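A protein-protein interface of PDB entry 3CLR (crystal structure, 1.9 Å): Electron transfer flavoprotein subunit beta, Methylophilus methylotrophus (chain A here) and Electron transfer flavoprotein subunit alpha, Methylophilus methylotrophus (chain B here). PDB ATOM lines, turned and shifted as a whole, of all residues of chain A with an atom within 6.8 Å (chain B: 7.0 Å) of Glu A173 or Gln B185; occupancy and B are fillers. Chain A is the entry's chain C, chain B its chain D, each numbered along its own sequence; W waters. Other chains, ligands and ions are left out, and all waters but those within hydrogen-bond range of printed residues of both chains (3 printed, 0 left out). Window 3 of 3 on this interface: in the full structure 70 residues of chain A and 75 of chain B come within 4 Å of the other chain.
Printed residues of chain B within 4 Å of Glu A173: Ser B184 and Gln B185. Of the printed residues of chain A, Gln B185 touches Val A172 (3.5 Å) and Glu A173 (2.9 Å). Of the printed residues of chain B, Ile A174 touches Arg B183 (3.9 Å) and Ser B184 (3.95 Å). Printed residues of chain A within 4 Å of Ser B184: Val A172, Glu A173 and Ile A174. Printed residues of chain A within 4 Å of Lys B187: Glu A171 (2.7 Å). Of the printed residues of chain B, Glu A171 touches Asn B186 (3.7 Å) and Lys B187 (2.7 Å). Printed residues of chain B within 4 Å of Val A172: Ser B184 (3.6 Å), Gln B185 (3.5 Å) and Asn B186 (3.6 Å). The nearest printed residue of chain B that does not touch Glu A173 is Lys B187 (4.2 Å). The nearest printed residue of chain A that does not touch Gln B185 is Glu A171 (4.5 Å).
The backbone carbonyl oxygen (O) of Ala A158 is in hydrogen-bond range of the backbone NH (N) of Ile A174, 2.8 Å away. The backbone carbonyl oxygen (O) of Val A172 sits at hydrogen-bond distance from the backbone NH (N) of Ile A160, at 2.8 Å. The side-chain hydroxyl of Ser B182 sits at hydrogen-bond distance from the backbone carbonyl oxygen of Ser B184 (3.0 Å).
Printed residues of chain B that touch a printed residue of chain A: Arg B183, Ser B184, Gln B185, Asn B186 and Lys B187. Along chain A the printed residues that touch a printed residue of chain B span positions 171 to 175. Among the printed residues, 10 pairs touch across the chains.
N of Asn A175 sits at hydrogen-bond distance from O of Arg B183, 3.0 Å away. The backbone carbonyl oxygen of Glu A173 is in hydrogen-bond range of the backbone NH of Gln B185 (2.9 Å). O of Glu A171 is in hydrogen-bond range of N of Lys B187 (2.7 Å).
Asn B186 touches Glu A171. Ser B184 touches Val A172. O of Gln B185 touches CA of Val A172, at 3.5 Å. Asn B186 touches Val A172 (OD1 to CG2, 3.6 Å). Glu A173 touches Ser B184 (O to CA, 3.2 Å). Ile A174 touches Arg B183 (CA to O, 3.9 Å). Ser B184 touches Ile A174.
Water W2 bridges the side-chain carboxylate (OE2) of Glu A173 (2.7 Å) and the side-chain amino group (NZ) of Lys B187 (2.8 Å). Water W3 lies within hydrogen-bond range of the side-chain amide nitrogen of Asn A175, the backbone carbonyl oxygen of Arg B183 and the backbone carbonyl oxygen of Glu A173. Water W1 lies within hydrogen-bond range of the backbone carbonyl oxygen of Ser B182 (3.1 Å) and the side-chain amide oxygen of Asn A175 (3.2 Å).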
ATOM      1  N   LYS A 157      -5.396   0.643  14.933  1.00  0.00           N
ATOM      2  CA  LYS A 157      -6.024  -0.613  14.551  1.00  0.00           C
ATOM      3  C   LYS A 157      -4.953  -1.692  14.395  1.00  0.00           C
ATOM      4  O   LYS A 157      -3.777  -1.389  14.124  1.00  0.00           O
ATOM      5  CB  LYS A 157      -6.833  -0.493  13.264  1.00  0.00           C
ATOM      6  CG  LYS A 157      -8.120   0.396  13.343  1.00  0.00           C
ATOM      7  N   ALA A 158      -5.357  -2.939  14.619  1.00  0.00           N
ATOM      8  CA  ALA A 158      -4.507  -4.127  14.389  1.00  0.00           C
ATOM      9  C   ALA A 158      -5.313  -5.105  13.559  1.00  0.00           C
ATOM     10  O   ALA A 158      -6.532  -5.012  13.505  1.00  0.00           O
ATOM     11  CB  ALA A 158      -4.101  -4.771  15.710  1.00  0.00           C
ATOM     12  N   VAL A 159      -4.638  -6.013  12.871  1.00  0.00           N
ATOM     13  CA  VAL A 159      -5.340  -7.093  12.208  1.00  0.00           C
ATOM     14  C   VAL A 159      -4.929  -8.386  12.845  1.00  0.00           C
ATOM     15  O   VAL A 159      -3.726  -8.716  12.962  1.00  0.00           O
ATOM     16  CB  VAL A 159      -5.091  -7.104  10.690  1.00  0.00           C
ATOM     17  CG1 VAL A 159      -5.824  -8.286  10.025  1.00  0.00           C
ATOM     18  CG2 VAL A 159      -5.591  -5.818  10.083  1.00  0.00           C
ATOM     19  N   ILE A 160      -5.930  -9.127  13.291  1.00  0.00           N
ATOM     20  CA  ILE A 160      -5.693 -10.418  13.921  1.00  0.00           C
ATOM     21  C   ILE A 160      -6.292 -11.498  13.091  1.00  0.00           C
ATOM     22  O   ILE A 160      -7.138 -11.223  12.249  1.00  0.00           O
ATOM     23  CB  ILE A 160      -6.203 -10.494  15.404  1.00  0.00           C
ATOM     24  CG1 ILE A 160      -7.716 -10.250  15.543  1.00  0.00           C
ATOM     25  CG2 ILE A 160      -5.419  -9.501  16.296  1.00  0.00           C
ATOM     26  CD1 ILE A 160      -8.537 -11.522  15.617  1.00  0.00           C
ATOM     27  N   GLU A 171      -9.719 -13.312   9.607  1.00  0.00           N
ATOM     28  CA  GLU A 171      -9.094 -12.024   9.821  1.00  0.00           C
ATOM     29  C   GLU A 171     -10.120 -11.075  10.410  1.00  0.00           C
ATOM     30  O   GLU A 171     -11.296 -11.028   9.957  1.00  0.00           O
ATOM     31  CB  GLU A 171      -8.548 -11.426   8.514  1.00  0.00           C
ATOM     32  CG  GLU A 171      -7.311 -12.121   8.082  1.00  0.00           C
ATOM     33  CD  GLU A 171      -6.556 -11.378   7.058  1.00  0.00           C
ATOM     34  OE1 GLU A 171      -7.042 -11.349   5.906  1.00  0.00           O
ATOM     35  OE2 GLU A 171      -5.478 -10.849   7.422  1.00  0.00           O
ATOM     36  N   VAL A 172      -9.656 -10.289  11.384  1.00  0.00           N
ATOM     37  CA  VAL A 172     -10.490  -9.300  12.062  1.00  0.00           C
ATOM     38  C   VAL A 172      -9.619  -8.058  12.264  1.00  0.00           C
ATOM     39  O   VAL A 172      -8.503  -8.168  12.752  1.00  0.00           O
ATOM     40  CB  VAL A 172     -11.009  -9.819  13.445  1.00  0.00           C
ATOM     41  CG1 VAL A 172     -11.853  -8.737  14.163  1.00  0.00           C
ATOM     42  CG2 VAL A 172     -11.844 -11.120  13.325  1.00  0.00           C
ATOM     43  N   GLU A 173     -10.119  -6.894  11.867  1.00  0.00           N
ATOM     44  CA  GLU A 173      -9.449  -5.622  12.137  1.00  0.00           C
ATOM     45  C   GLU A 173     -10.048  -5.084  13.404  1.00  0.00           C
ATOM     46  O   GLU A 173     -11.260  -4.937  13.502  1.00  0.00           O
ATOM     47  CB  GLU A 173      -9.665  -4.635  11.007  1.00  0.00           C
ATOM     48  CG  GLU A 173      -8.902  -3.329  11.198  1.00  0.00           C
ATOM     49  CD  GLU A 173      -8.948  -2.517   9.920  1.00  0.00           C
ATOM     50  OE1 GLU A 173      -7.919  -2.464   9.208  1.00  0.00           O
ATOM     51  OE2 GLU A 173     -10.043  -2.009   9.622  1.00  0.00           O
ATOM     52  N   ILE A 174      -9.197  -4.771  14.375  1.00  0.00           N
ATOM     53  CA  ILE A 174      -9.651  -4.432  15.698  1.00  0.00           C
ATOM     54  C   ILE A 174      -9.048  -3.105  16.162  1.00  0.00           C
ATOM     55  O   ILE A 174      -7.871  -2.844  15.950  1.00  0.00           O
ATOM     56  CB  ILE A 174      -9.355  -5.628  16.684  1.00  0.00           C
ATOM     57  CG1 ILE A 174      -9.951  -5.355  18.068  1.00  0.00           C
ATOM     58  CG2 ILE A 174      -7.837  -5.958  16.738  1.00  0.00           C
ATOM     59  CD1 ILE A 174      -9.997  -6.547  18.973  1.00  0.00           C
ATOM     60  N   ASN A 175      -9.887  -2.238  16.735  1.00  0.00           N
ATOM     61  CA  ASN A 175      -9.420  -1.019  17.381  1.00  0.00           C
ATOM     62  C   ASN A 175      -8.427  -1.321  18.511  1.00  0.00           C
ATOM     63  O   ASN A 175      -8.617  -2.258  19.315  1.00  0.00           O
ATOM     64  CB  ASN A 175     -10.581  -0.223  17.997  1.00  0.00           C
ATOM     65  CG  ASN A 175     -11.594   0.299  16.975  1.00  0.00           C
ATOM     66  OD1 ASN A 175     -12.597   0.897  17.371  1.00  0.00           O
ATOM     67  ND2 ASN A 175     -11.349   0.091  15.687  1.00  0.00           N
ATOM     68  N   SER B  67     -25.351  -5.826  13.011  1.00  0.00           N
ATOM     69  CA  SER B  67     -24.583  -5.186  11.965  1.00  0.00           C
ATOM     70  C   SER B  67     -23.653  -6.140  11.195  1.00  0.00           C
ATOM     71  O   SER B  67     -23.239  -5.798  10.104  1.00  0.00           O
ATOM     72  CB  SER B  67     -23.760  -4.051  12.577  1.00  0.00           C
ATOM     73  OG  SER B  67     -22.935  -4.524  13.629  1.00  0.00           O
ATOM     74  N   SER B  68     -23.297  -7.305  11.750  1.00  0.00           N
ATOM     75  CA  SER B  68     -22.368  -8.215  11.073  1.00  0.00           C
ATOM     76  C   SER B  68     -23.050  -9.480  10.588  1.00  0.00           C
ATOM     77  O   SER B  68     -24.080  -9.878  11.118  1.00  0.00           O
ATOM     78  CB  SER B  68     -21.186  -8.590  11.971  1.00  0.00           C
ATOM     79  OG  SER B  68     -21.623  -9.273  13.118  1.00  0.00           O
ATOM     80  N   ASP B  72     -19.543 -11.396  15.869  1.00  0.00           N
ATOM     81  CA  ASP B  72     -18.841 -10.218  16.322  1.00  0.00           C
ATOM     82  C   ASP B  72     -19.080 -10.146  17.838  1.00  0.00           C
ATOM     83  O   ASP B  72     -20.223 -10.216  18.296  1.00  0.00           O
ATOM     84  CB  ASP B  72     -19.385  -8.985  15.610  1.00  0.00           C
ATOM     85  CG  ASP B  72     -18.806  -7.700  16.149  1.00  0.00           C
ATOM     86  OD1 ASP B  72     -19.135  -7.301  17.301  1.00  0.00           O
ATOM     87  OD2 ASP B  72     -18.010  -7.105  15.415  1.00  0.00           O
ATOM     88  N   SER B 182     -19.643  -1.724  16.510  1.00  0.00           N
ATOM     89  CA  SER B 182     -18.604  -2.636  16.975  1.00  0.00           C
ATOM     90  C   SER B 182     -17.234  -2.002  16.908  1.00  0.00           C
ATOM     91  O   SER B 182     -16.953  -1.163  16.038  1.00  0.00           O
ATOM     92  CB  SER B 182     -18.606  -3.919  16.155  1.00  0.00           C
ATOM     93  OG  SER B 182     -17.556  -4.775  16.594  1.00  0.00           O
ATOM     94  N   ARG B 183     -16.359  -2.428  17.812  1.00  0.00           N
ATOM     95  CA  ARG B 183     -14.998  -1.967  17.831  1.00  0.00           C
ATOM     96  C   ARG B 183     -14.034  -2.842  17.021  1.00  0.00           C
ATOM     97  O   ARG B 183     -12.800  -2.683  17.121  1.00  0.00           O
ATOM     98  CB  ARG B 183     -14.538  -1.818  19.264  1.00  0.00           C
ATOM     99  CG  ARG B 183     -15.302  -0.688  19.973  1.00  0.00           C
ATOM    100  CD  ARG B 183     -15.132  -0.764  21.490  1.00  0.00           C
ATOM    101  NE  ARG B 183     -15.682  -1.994  21.993  1.00  0.00           N
ATOM    102  CZ  ARG B 183     -15.737  -2.329  23.271  1.00  0.00           C
ATOM    103  NH1 ARG B 183     -15.284  -1.506  24.191  1.00  0.00           N
ATOM    104  NH2 ARG B 183     -16.288  -3.479  23.612  1.00  0.00           N
ATOM    105  N   SER B 184     -14.604  -3.768  16.249  1.00  0.00           N
ATOM    106  CA  SER B 184     -13.868  -4.539  15.279  1.00  0.00           C
ATOM    107  C   SER B 184     -14.717  -4.774  14.028  1.00  0.00           C
ATOM    108  O   SER B 184     -15.940  -4.580  14.051  1.00  0.00           O
ATOM    109  CB  SER B 184     -13.328  -5.876  15.876  1.00  0.00           C
ATOM    110  OG  SER B 184     -14.349  -6.763  16.295  1.00  0.00           O
ATOM    111  N   GLN B 185     -14.056  -5.096  12.921  1.00  0.00           N
ATOM    112  CA  GLN B 185     -14.732  -5.521  11.695  1.00  0.00           C
ATOM    113  C   GLN B 185     -14.114  -6.805  11.185  1.00  0.00           C
ATOM    114  O   GLN B 185     -12.904  -6.951  11.124  1.00  0.00           O
ATOM    115  CB  GLN B 185     -14.679  -4.459  10.597  1.00  0.00           C
ATOM    116  CG  GLN B 185     -14.863  -5.024   9.153  1.00  0.00           C
ATOM    117  CD  GLN B 185     -16.320  -5.120   8.661  1.00  0.00           C
ATOM    118  OE1 GLN B 185     -17.059  -4.142   8.723  1.00  0.00           O
ATOM    119  NE2 GLN B 185     -16.705  -6.281   8.114  1.00  0.00           N
ATOM    120  N   ASN B 186     -14.984  -7.725  10.805  1.00  0.00           N
ATOM    121  CA  ASN B 186     -14.577  -9.014  10.292  1.00  0.00           C
ATOM    122  C   ASN B 186     -14.106  -8.854   8.842  1.00  0.00           C
ATOM    123  O   ASN B 186     -14.697  -8.109   8.042  1.00  0.00           O
ATOM    124  CB  ASN B 186     -15.736  -9.987  10.349  1.00  0.00           C
ATOM    125  CG  ASN B 186     -16.115 -10.387  11.768  1.00  0.00           C
ATOM    126  OD1 ASN B 186     -15.322 -10.229  12.729  1.00  0.00           O
ATOM    127  ND2 ASN B 186     -17.336 -10.943  11.905  1.00  0.00           N
ATOM    128  N   LYS B 187     -13.043  -9.566   8.505  1.00  0.00           N
ATOM    129  CA  LYS B 187     -12.517  -9.539   7.164  1.00  0.00           C
ATOM    130  C   LYS B 187     -12.562 -10.938   6.576  1.00  0.00           C
ATOM    131  O   LYS B 187     -13.520 -11.677   6.849  1.00  0.00           O
ATOM    132  CB  LYS B 187     -11.151  -8.873   7.167  1.00  0.00           C
ATOM    133  CG  LYS B 187     -11.183  -7.469   7.766  1.00  0.00           C
ATOM    134  CD  LYS B 187     -11.981  -6.488   6.900  1.00  0.00           C
ATOM    135  CE  LYS B 187     -11.791  -5.059   7.384  1.00  0.00           C
ATOM    136  NZ  LYS B 187     -12.556  -4.049   6.590  1.00  0.00           N
HETATM  137  O   HOH W   1     -15.400   1.504  15.891  1.00  0.00           O
HETATM  138  O   HOH W   2     -11.615  -1.521   7.455  1.00  0.00           O
HETATM  139  O   HOH W   3     -12.332  -1.811  13.940  1.00  0.00           O
